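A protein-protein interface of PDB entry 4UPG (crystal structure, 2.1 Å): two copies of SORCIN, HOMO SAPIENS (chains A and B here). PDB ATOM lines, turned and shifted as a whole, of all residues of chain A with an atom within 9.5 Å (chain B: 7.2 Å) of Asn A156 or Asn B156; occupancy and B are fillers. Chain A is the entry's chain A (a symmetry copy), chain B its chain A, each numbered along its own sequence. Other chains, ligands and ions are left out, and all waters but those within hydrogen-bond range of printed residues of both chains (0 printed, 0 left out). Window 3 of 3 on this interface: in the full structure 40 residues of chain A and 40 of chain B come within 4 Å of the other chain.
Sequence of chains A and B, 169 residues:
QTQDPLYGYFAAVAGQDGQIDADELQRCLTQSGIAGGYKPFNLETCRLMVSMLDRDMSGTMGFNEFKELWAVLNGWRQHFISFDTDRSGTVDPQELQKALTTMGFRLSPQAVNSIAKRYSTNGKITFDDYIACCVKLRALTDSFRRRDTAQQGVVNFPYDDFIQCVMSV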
ATOM      1  N   SER A 143     -26.893  24.158  -0.342  1.00  0.00           N
ATOM      2  CA  SER A 143     -25.805  23.408  -1.004  1.00  0.00           C
ATOM      3  C   SER A 143     -24.531  23.432  -0.180  1.00  0.00           C
ATOM      4  O   SER A 143     -23.843  22.420  -0.008  1.00  0.00           O
ATOM      5  CB  SER A 143     -25.542  23.969  -2.411  1.00  0.00           C
ATOM      6  OG  SER A 143     -26.639  23.695  -3.257  1.00  0.00           O
ATOM      7  N   PHE A 144     -24.226  24.596   0.376  1.00  0.00           N
ATOM      8  CA  PHE A 144     -23.024  24.747   1.176  1.00  0.00           C
ATOM      9  C   PHE A 144     -23.140  23.925   2.464  1.00  0.00           C
ATOM     10  O   PHE A 144     -22.267  23.107   2.762  1.00  0.00           O
ATOM     11  CB  PHE A 144     -22.801  26.219   1.500  1.00  0.00           C
ATOM     12  CG  PHE A 144     -21.504  26.501   2.168  1.00  0.00           C
ATOM     13  CD1 PHE A 144     -21.381  26.393   3.559  1.00  0.00           C
ATOM     14  CD2 PHE A 144     -20.401  26.932   1.424  1.00  0.00           C
ATOM     15  CE1 PHE A 144     -20.182  26.686   4.185  1.00  0.00           C
ATOM     16  CE2 PHE A 144     -19.191  27.199   2.042  1.00  0.00           C
ATOM     17  CZ  PHE A 144     -19.083  27.085   3.426  1.00  0.00           C
ATOM     18  N   ARG A 147     -22.773  20.211   2.237  1.00  0.00           N
ATOM     19  CA  ARG A 147     -21.403  19.768   2.031  1.00  0.00           C
ATOM     20  C   ARG A 147     -20.520  20.006   3.249  1.00  0.00           C
ATOM     21  O   ARG A 147     -19.436  19.438   3.352  1.00  0.00           O
ATOM     22  CB  ARG A 147     -20.801  20.500   0.825  1.00  0.00           C
ATOM     23  CG  ARG A 147     -21.326  20.004  -0.504  1.00  0.00           C
ATOM     24  CD  ARG A 147     -20.995  20.970  -1.636  1.00  0.00           C
ATOM     25  NE  ARG A 147     -21.441  20.430  -2.917  1.00  0.00           N
ATOM     26  CZ  ARG A 147     -22.713  20.386  -3.331  1.00  0.00           C
ATOM     27  NH1 ARG A 147     -23.721  20.855  -2.573  1.00  0.00           N
ATOM     28  NH2 ARG A 147     -22.973  19.841  -4.507  1.00  0.00           N
ATOM     29  N   ASP A 148     -20.940  20.878   4.153  1.00  0.00           N
ATOM     30  CA  ASP A 148     -20.093  21.243   5.300  1.00  0.00           C
ATOM     31  C   ASP A 148     -20.344  20.217   6.421  1.00  0.00           C
ATOM     32  O   ASP A 148     -20.942  20.540   7.454  1.00  0.00           O
ATOM     33  CB  ASP A 148     -20.478  22.654   5.758  1.00  0.00           C
ATOM     34  CG  ASP A 148     -19.577  23.198   6.862  1.00  0.00           C
ATOM     35  OD1 ASP A 148     -18.488  22.643   7.110  1.00  0.00           O
ATOM     36  OD2 ASP A 148     -19.987  24.187   7.470  1.00  0.00           O
ATOM     37  N   THR A 149     -19.927  18.980   6.186  1.00  0.00           N
ATOM     38  CA  THR A 149     -20.190  17.858   7.101  1.00  0.00           C
ATOM     39  C   THR A 149     -19.527  18.023   8.489  1.00  0.00           C
ATOM     40  O   THR A 149     -20.054  17.530   9.473  1.00  0.00           O
ATOM     41  CB  THR A 149     -19.766  16.505   6.488  1.00  0.00           C
ATOM     42  OG1 THR A 149     -18.542  16.662   5.793  1.00  0.00           O
ATOM     43  CG2 THR A 149     -20.793  16.040   5.464  1.00  0.00           C
ATOM     44  N   ALA A 150     -18.422  18.757   8.539  1.00  0.00           N
ATOM     45  CA  ALA A 150     -17.685  19.024   9.750  1.00  0.00           C
ATOM     46  C   ALA A 150     -18.184  20.282  10.422  1.00  0.00           C
ATOM     47  O   ALA A 150     -17.673  20.654  11.461  1.00  0.00           O
ATOM     48  CB  ALA A 150     -16.188  19.158   9.427  1.00  0.00           C
ATOM     49  N   GLN A 152     -17.643  23.416   9.858  1.00  0.00           N
ATOM     50  CA  GLN A 152     -16.590  24.442  10.038  1.00  0.00           C
ATOM     51  C   GLN A 152     -16.865  25.764   9.349  1.00  0.00           C
ATOM     52  O   GLN A 152     -16.090  26.691   9.486  1.00  0.00           O
ATOM     53  CB  GLN A 152     -15.274  23.919   9.453  1.00  0.00           C
ATOM     54  CG  GLN A 152     -14.836  22.596  10.030  1.00  0.00           C
ATOM     55  CD  GLN A 152     -14.551  22.724  11.501  1.00  0.00           C
ATOM     56  OE1 GLN A 152     -15.152  22.039  12.329  1.00  0.00           O
ATOM     57  NE2 GLN A 152     -13.638  23.618  11.841  1.00  0.00           N
ATOM     58  N   GLY A 153     -17.924  25.849   8.554  1.00  0.00           N
ATOM     59  CA  GLY A 153     -18.221  27.085   7.806  1.00  0.00           C
ATOM     60  C   GLY A 153     -17.304  27.278   6.602  1.00  0.00           C
ATOM     61  O   GLY A 153     -17.229  28.369   6.010  1.00  0.00           O
ATOM     62  N   VAL A 154     -16.591  26.216   6.245  1.00  0.00           N
ATOM     63  CA  VAL A 154     -15.718  26.216   5.082  1.00  0.00           C
ATOM     64  C   VAL A 154     -16.010  24.893   4.382  1.00  0.00           C
ATOM     65  O   VAL A 154     -16.194  23.870   5.048  1.00  0.00           O
ATOM     66  CB  VAL A 154     -14.204  26.361   5.455  1.00  0.00           C
ATOM     67  CG1 VAL A 154     -13.962  27.547   6.382  1.00  0.00           C
ATOM     68  CG2 VAL A 154     -13.678  25.090   6.101  1.00  0.00           C
ATOM     69  N   VAL A 155     -16.112  24.921   3.057  1.00  0.00           N
ATOM     70  CA  VAL A 155     -16.371  23.726   2.251  1.00  0.00           C
ATOM     71  C   VAL A 155     -15.274  23.597   1.220  1.00  0.00           C
ATOM     72  O   VAL A 155     -14.902  24.580   0.564  1.00  0.00           O
ATOM     73  CB  VAL A 155     -17.745  23.774   1.525  1.00  0.00           C
ATOM     74  CG1 VAL A 155     -17.858  22.698   0.444  1.00  0.00           C
ATOM     75  CG2 VAL A 155     -18.876  23.610   2.511  1.00  0.00           C
ATOM     76  N   ASN A 156     -14.759  22.384   1.096  1.00  0.00           N
ATOM     77  CA  ASN A 156     -13.798  22.021   0.056  1.00  0.00           C
ATOM     78  C   ASN A 156     -14.483  21.600  -1.203  1.00  0.00           C
ATOM     79  O   ASN A 156     -14.983  20.489  -1.291  1.00  0.00           O
ATOM     80  CB  ASN A 156     -12.966  20.824   0.494  1.00  0.00           C
ATOM     81  CG  ASN A 156     -11.605  21.220   0.952  1.00  0.00           C
ATOM     82  OD1 ASN A 156     -10.594  20.926   0.284  1.00  0.00           O
ATOM     83  ND2 ASN A 156     -11.554  21.935   2.074  1.00  0.00           N
ATOM     84  N   PHE A 157     -14.435  22.456  -2.215  1.00  0.00           N
ATOM     85  CA  PHE A 157     -15.184  22.238  -3.440  1.00  0.00           C
ATOM     86  C   PHE A 157     -14.250  21.807  -4.537  1.00  0.00           C
ATOM     87  O   PHE A 157     -13.387  22.601  -4.954  1.00  0.00           O
ATOM     88  CB  PHE A 157     -15.783  23.564  -3.888  1.00  0.00           C
ATOM     89  CG  PHE A 157     -17.173  23.804  -3.435  1.00  0.00           C
ATOM     90  CD1 PHE A 157     -18.232  23.200  -4.085  1.00  0.00           C
ATOM     91  CD2 PHE A 157     -17.431  24.699  -2.412  1.00  0.00           C
ATOM     92  CE1 PHE A 157     -19.557  23.478  -3.700  1.00  0.00           C
ATOM     93  CE2 PHE A 157     -18.742  24.964  -2.020  1.00  0.00           C
ATOM     94  CZ  PHE A 157     -19.791  24.358  -2.679  1.00  0.00           C
ATOM     95  N   PRO A 158     -14.423  20.574  -5.043  1.00  0.00           N
ATOM     96  CA  PRO A 158     -13.807  20.306  -6.336  1.00  0.00           C
ATOM     97  C   PRO A 158     -14.466  21.152  -7.415  1.00  0.00           C
ATOM     98  O   PRO A 158     -15.674  21.452  -7.325  1.00  0.00           O
ATOM     99  CB  PRO A 158     -14.089  18.820  -6.581  1.00  0.00           C
ATOM    100  CG  PRO A 158     -14.547  18.267  -5.275  1.00  0.00           C
ATOM    101  CD  PRO A 158     -15.186  19.412  -4.546  1.00  0.00           C
ATOM    102  N   TYR A 159     -13.676  21.485  -8.435  1.00  0.00           N
ATOM    103  CA  TYR A 159     -14.117  22.337  -9.540  1.00  0.00           C
ATOM    104  C   TYR A 159     -15.430  21.869 -10.183  1.00  0.00           C
ATOM    105  O   TYR A 159     -16.355  22.671 -10.321  1.00  0.00           O
ATOM    106  CB  TYR A 159     -13.031  22.421 -10.635  1.00  0.00           C
ATOM    107  CG  TYR A 159     -13.489  23.187 -11.853  1.00  0.00           C
ATOM    108  CD1 TYR A 159     -13.693  24.570 -11.797  1.00  0.00           C
ATOM    109  CD2 TYR A 159     -13.770  22.526 -13.054  1.00  0.00           C
ATOM    110  CE1 TYR A 159     -14.151  25.274 -12.905  1.00  0.00           C
ATOM    111  CE2 TYR A 159     -14.251  23.222 -14.162  1.00  0.00           C
ATOM    112  CZ  TYR A 159     -14.419  24.595 -14.092  1.00  0.00           C
ATOM    113  OH  TYR A 159     -14.874  25.268 -15.223  1.00  0.00           O
ATOM    114  N   ASP A 160     -15.528  20.598 -10.600  1.00  0.00           N
ATOM    115  CA  ASP A 160     -16.718  20.196 -11.358  1.00  0.00           C
ATOM    116  C   ASP A 160     -17.975  20.176 -10.465  1.00  0.00           C
ATOM    117  O   ASP A 160     -19.029  20.557 -10.926  1.00  0.00           O
ATOM    118  CB  ASP A 160     -16.488  18.897 -12.161  1.00  0.00           C
ATOM    119  CG  ASP A 160     -16.004  19.181 -13.600  1.00  0.00           C
ATOM    120  OD1 ASP A 160     -16.765  19.792 -14.387  1.00  0.00           O
ATOM    121  OD2 ASP A 160     -14.871  18.817 -13.948  1.00  0.00           O
ATOM    122  N   ASP A 161     -17.842  19.777  -9.196  1.00  0.00           N
ATOM    123  CA  ASP A 161     -18.930  19.865  -8.222  1.00  0.00           C
ATOM    124  C   ASP A 161     -19.365  21.337  -7.994  1.00  0.00           C
ATOM    125  O   ASP A 161     -20.566  21.651  -7.972  1.00  0.00           O
ATOM    126  CB  ASP A 161     -18.534  19.199  -6.897  1.00  0.00           C
ATOM    127  CG  ASP A 161     -19.634  19.346  -5.816  1.00  0.00           C
ATOM    128  OD1 ASP A 161     -20.818  18.948  -6.052  1.00  0.00           O
ATOM    129  OD2 ASP A 161     -19.353  19.951  -4.755  1.00  0.00           O
ATOM    130  N   PHE A 162     -18.378  22.238  -7.862  1.00  0.00           N
ATOM    131  CA  PHE A 162     -18.634  23.684  -7.755  1.00  0.00           C
ATOM    132  C   PHE A 162     -19.459  24.166  -8.954  1.00  0.00           C
ATOM    133  O   PHE A 162     -20.528  24.805  -8.801  1.00  0.00           O
ATOM    134  CB  PHE A 162     -17.280  24.437  -7.606  1.00  0.00           C
ATOM    135  CG  PHE A 162     -17.384  25.939  -7.614  1.00  0.00           C
ATOM    136  CD1 PHE A 162     -17.820  26.625  -6.501  1.00  0.00           C
ATOM    137  CD2 PHE A 162     -16.993  26.679  -8.729  1.00  0.00           C
ATOM    138  CE1 PHE A 162     -17.915  28.005  -6.508  1.00  0.00           C
ATOM    139  CE2 PHE A 162     -17.075  28.081  -8.730  1.00  0.00           C
ATOM    140  CZ  PHE A 162     -17.532  28.734  -7.630  1.00  0.00           C
ATOM    141  N   PHE B 144     -12.840  30.565  -9.324  1.00  0.00           N
ATOM    142  CA  PHE B 144     -12.310  29.341  -8.749  1.00  0.00           C
ATOM    143  C   PHE B 144     -10.787  29.294  -8.923  1.00  0.00           C
ATOM    144  O   PHE B 144     -10.054  29.118  -7.947  1.00  0.00           O
ATOM    145  CB  PHE B 144     -12.962  28.135  -9.413  1.00  0.00           C
ATOM    146  CG  PHE B 144     -12.616  26.837  -8.779  1.00  0.00           C
ATOM    147  CD1 PHE B 144     -11.454  26.149  -9.151  1.00  0.00           C
ATOM    148  CD2 PHE B 144     -13.474  26.254  -7.841  1.00  0.00           C
ATOM    149  CE1 PHE B 144     -11.147  24.925  -8.584  1.00  0.00           C
ATOM    150  CE2 PHE B 144     -13.159  25.042  -7.249  1.00  0.00           C
ATOM    151  CZ  PHE B 144     -11.998  24.372  -7.627  1.00  0.00           C
ATOM    152  N   ARG B 147      -8.683  31.478  -6.736  1.00  0.00           N
ATOM    153  CA  ARG B 147      -8.582  31.009  -5.363  1.00  0.00           C
ATOM    154  C   ARG B 147      -7.773  29.724  -5.240  1.00  0.00           C
ATOM    155  O   ARG B 147      -7.348  29.359  -4.147  1.00  0.00           O
ATOM    156  CB  ARG B 147      -9.986  30.774  -4.793  1.00  0.00           C
ATOM    157  CG  ARG B 147     -10.726  32.052  -4.467  1.00  0.00           C
ATOM    158  CD  ARG B 147     -12.214  31.803  -4.253  1.00  0.00           C
ATOM    159  NE  ARG B 147     -12.888  33.038  -3.860  1.00  0.00           N
ATOM    160  CZ  ARG B 147     -13.181  34.048  -4.686  1.00  0.00           C
ATOM    161  NH1 ARG B 147     -12.865  34.010  -5.993  1.00  0.00           N
ATOM    162  NH2 ARG B 147     -13.770  35.120  -4.184  1.00  0.00           N
ATOM    163  N   ASP B 148      -7.595  29.002  -6.335  1.00  0.00           N
ATOM    164  CA  ASP B 148      -6.920  27.695  -6.276  1.00  0.00           C
ATOM    165  C   ASP B 148      -5.403  27.938  -6.393  1.00  0.00           C
ATOM    166  O   ASP B 148      -4.785  27.601  -7.410  1.00  0.00           O
ATOM    167  CB  ASP B 148      -7.425  26.835  -7.439  1.00  0.00           C
ATOM    168  CG  ASP B 148      -6.895  25.405  -7.409  1.00  0.00           C
ATOM    169  OD1 ASP B 148      -6.364  24.957  -6.373  1.00  0.00           O
ATOM    170  OD2 ASP B 148      -7.022  24.748  -8.442  1.00  0.00           O
ATOM    171  N   VAL B 154      -9.257  22.000  -6.297  1.00  0.00           N
ATOM    172  CA  VAL B 154     -10.178  22.030  -5.172  1.00  0.00           C
ATOM    173  C   VAL B 154      -9.914  23.370  -4.494  1.00  0.00           C
ATOM    174  O   VAL B 154      -8.758  23.792  -4.390  1.00  0.00           O
ATOM    175  CB  VAL B 154      -9.982  20.827  -4.189  1.00  0.00           C
ATOM    176  CG1 VAL B 154      -9.983  19.492  -4.925  1.00  0.00           C
ATOM    177  CG2 VAL B 154      -8.694  20.975  -3.397  1.00  0.00           C
ATOM    178  N   VAL B 155     -10.975  24.064  -4.091  1.00  0.00           N
ATOM    179  CA  VAL B 155     -10.874  25.355  -3.410  1.00  0.00           C
ATOM    180  C   VAL B 155     -11.613  25.263  -2.095  1.00  0.00           C
ATOM    181  O   VAL B 155     -12.737  24.745  -2.036  1.00  0.00           O
ATOM    182  CB  VAL B 155     -11.468  26.525  -4.245  1.00  0.00           C
ATOM    183  CG1 VAL B 155     -11.656  27.788  -3.403  1.00  0.00           C
ATOM    184  CG2 VAL B 155     -10.582  26.842  -5.426  1.00  0.00           C
ATOM    185  N   ASN B 156     -10.967  25.757  -1.052  1.00  0.00           N
ATOM    186  CA  ASN B 156     -11.569  25.898   0.273  1.00  0.00           C
ATOM    187  C   ASN B 156     -12.299  27.194   0.410  1.00  0.00           C
ATOM    188  O   ASN B 156     -11.681  28.234   0.591  1.00  0.00           O
ATOM    189  CB  ASN B 156     -10.493  25.914   1.348  1.00  0.00           C
ATOM    190  CG  ASN B 156     -10.384  24.607   2.056  1.00  0.00           C
ATOM    191  OD1 ASN B 156     -10.736  24.493   3.247  1.00  0.00           O
ATOM    192  ND2 ASN B 156      -9.939  23.586   1.327  1.00  0.00           N
ATOM    193  N   PHE B 157     -13.624  27.129   0.410  1.00  0.00           N
ATOM    194  CA  PHE B 157     -14.451  28.323   0.386  1.00  0.00           C
ATOM    195  C   PHE B 157     -15.055  28.551   1.743  1.00  0.00           C
ATOM    196  O   PHE B 157     -15.878  27.731   2.193  1.00  0.00           O
ATOM    197  CB  PHE B 157     -15.616  28.089  -0.566  1.00  0.00           C
ATOM    198  CG  PHE B 157     -15.399  28.575  -1.949  1.00  0.00           C
ATOM    199  CD1 PHE B 157     -15.533  29.917  -2.244  1.00  0.00           C
ATOM    200  CD2 PHE B 157     -15.142  27.681  -2.972  1.00  0.00           C
ATOM    201  CE1 PHE B 157     -15.393  30.373  -3.569  1.00  0.00           C
ATOM    202  CE2 PHE B 157     -14.988  28.131  -4.281  1.00  0.00           C
ATOM    203  CZ  PHE B 157     -15.128  29.474  -4.565  1.00  0.00           C
ATOM    204  N   PRO B 158     -14.694  29.667   2.399  1.00  0.00           N
ATOM    205  CA  PRO B 158     -15.552  30.084   3.499  1.00  0.00           C
ATOM    206  C   PRO B 158     -16.920  30.493   2.972  1.00  0.00           C
ATOM    207  O   PRO B 158     -17.026  31.006   1.840  1.00  0.00           O
ATOM    208  CB  PRO B 158     -14.830  31.298   4.094  1.00  0.00           C
ATOM    209  CG  PRO B 158     -13.457  31.285   3.513  1.00  0.00           C
ATOM    210  CD  PRO B 158     -13.583  30.612   2.177  1.00  0.00           C
ATOM    211  N   ASP B 161     -17.457  34.290   1.650  1.00  0.00           N
ATOM    212  CA  ASP B 161     -16.737  34.431   0.384  1.00  0.00           C
ATOM    213  C   ASP B 161     -17.461  33.675  -0.762  1.00  0.00           C
ATOM    214  O   ASP B 161     -17.630  34.210  -1.871  1.00  0.00           O
ATOM    215  CB  ASP B 161     -15.286  33.953   0.524  1.00  0.00           C
ATOM    216  CG  ASP B 161     -14.517  34.010  -0.820  1.00  0.00           C
ATOM    217  OD1 ASP B 161     -14.452  35.101  -1.471  1.00  0.00           O
ATOM    218  OD2 ASP B 161     -14.055  32.946  -1.291  1.00  0.00           O
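The backbone carbonyl oxygen (O) of Val B155 lies close to the backbone carbonyl oxygen (O) of Val A155. The side-chain amide nitrogen (ND2) of Asn A156 lies close to the side-chain amide nitrogen (ND2) of Asn B156 (2.4 Å). The backbone NH (N) of Phe B157 lies within hydrogen-bond range of the backbone carbonyl oxygen (O) of Val A155, 2.9 Å away. The backbone carbonyl oxygen of Val B155 lies within hydrogen-bond range of the backbone NH of Phe A157 (2.9 Å).
OD2 of Asp A148 sits at hydrogen-bond distance from N of Gly A153 (2.9 Å).
Among the printed residues, merely in contact across the chains: Phe A144 with Phe B157 (3.4 Å), Gly A153 with Pro B158 (3.5 Å), Val A154 with Phe B157 (3.3 Å), Val A155 with Asn B156 (3.6 Å), Asn A156 with Val B155 (3.6 Å), Phe A157 with Phe B144 (3.4 Å), Phe A157 with Val B154 (3.3 Å), Phe A157 with Phe B157 (3.8 Å), Tyr A159 with Phe B144 (3.4 Å), Phe A162 with Phe B144 (3.7 Å) and Phe A162 with Phe B157 (3.7 Å).
Of the printed residues of chain B, Val A154 touches Phe B157 (3.3 Å). Of chain B, only Val B155 (3.6 Å) and Asn B156 (2.4 Å) come within 4 Å of Asn A156. Arg B147 touches none of the printed residues of chain A. Asp B148 touches none of the printed residues of chain A. Printed residues of chain A within 4 Å of Phe B157: Phe A144, Val A154, Val A155, Phe A157 and Phe A162. The nearest residue of chain B that does not touch Asn A156 is Val B154 (4.1 Å). The nearest residue of chain A that does not touch Asn B156 is Val A154 (4.1 Å).
Printed residues of chain B that touch a printed residue of chain A: Phe B144, Val B154, Val B155, Asn B156, Phe B157 and Pro B158. Among the printed residues, 15 pairs touch across the chains. Among the printed residues, no Asp or Glu carboxylate lies within 4 Å of a Lys or Arg side-chain nitrogen of the other chain.
Phe A144 touches Phe B157, and with the chains exchanged Phe A157 touches Phe B144. Val A155 touches Asn B156, and with the chains exchanged Asn A156 touches Val B155. Val A155 touches Phe B157, and with the chains exchanged Phe A157 touches Val B155. Phe B157 touches its own counterpart, Phe A157. Positions printed for both chains: 144, 147, 148, 154, 155, 156, 157, 158 and 161. Of the 15 pairs that touch across the chains among the printed residues, 11 have their exchanged pair printed and touching as well.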
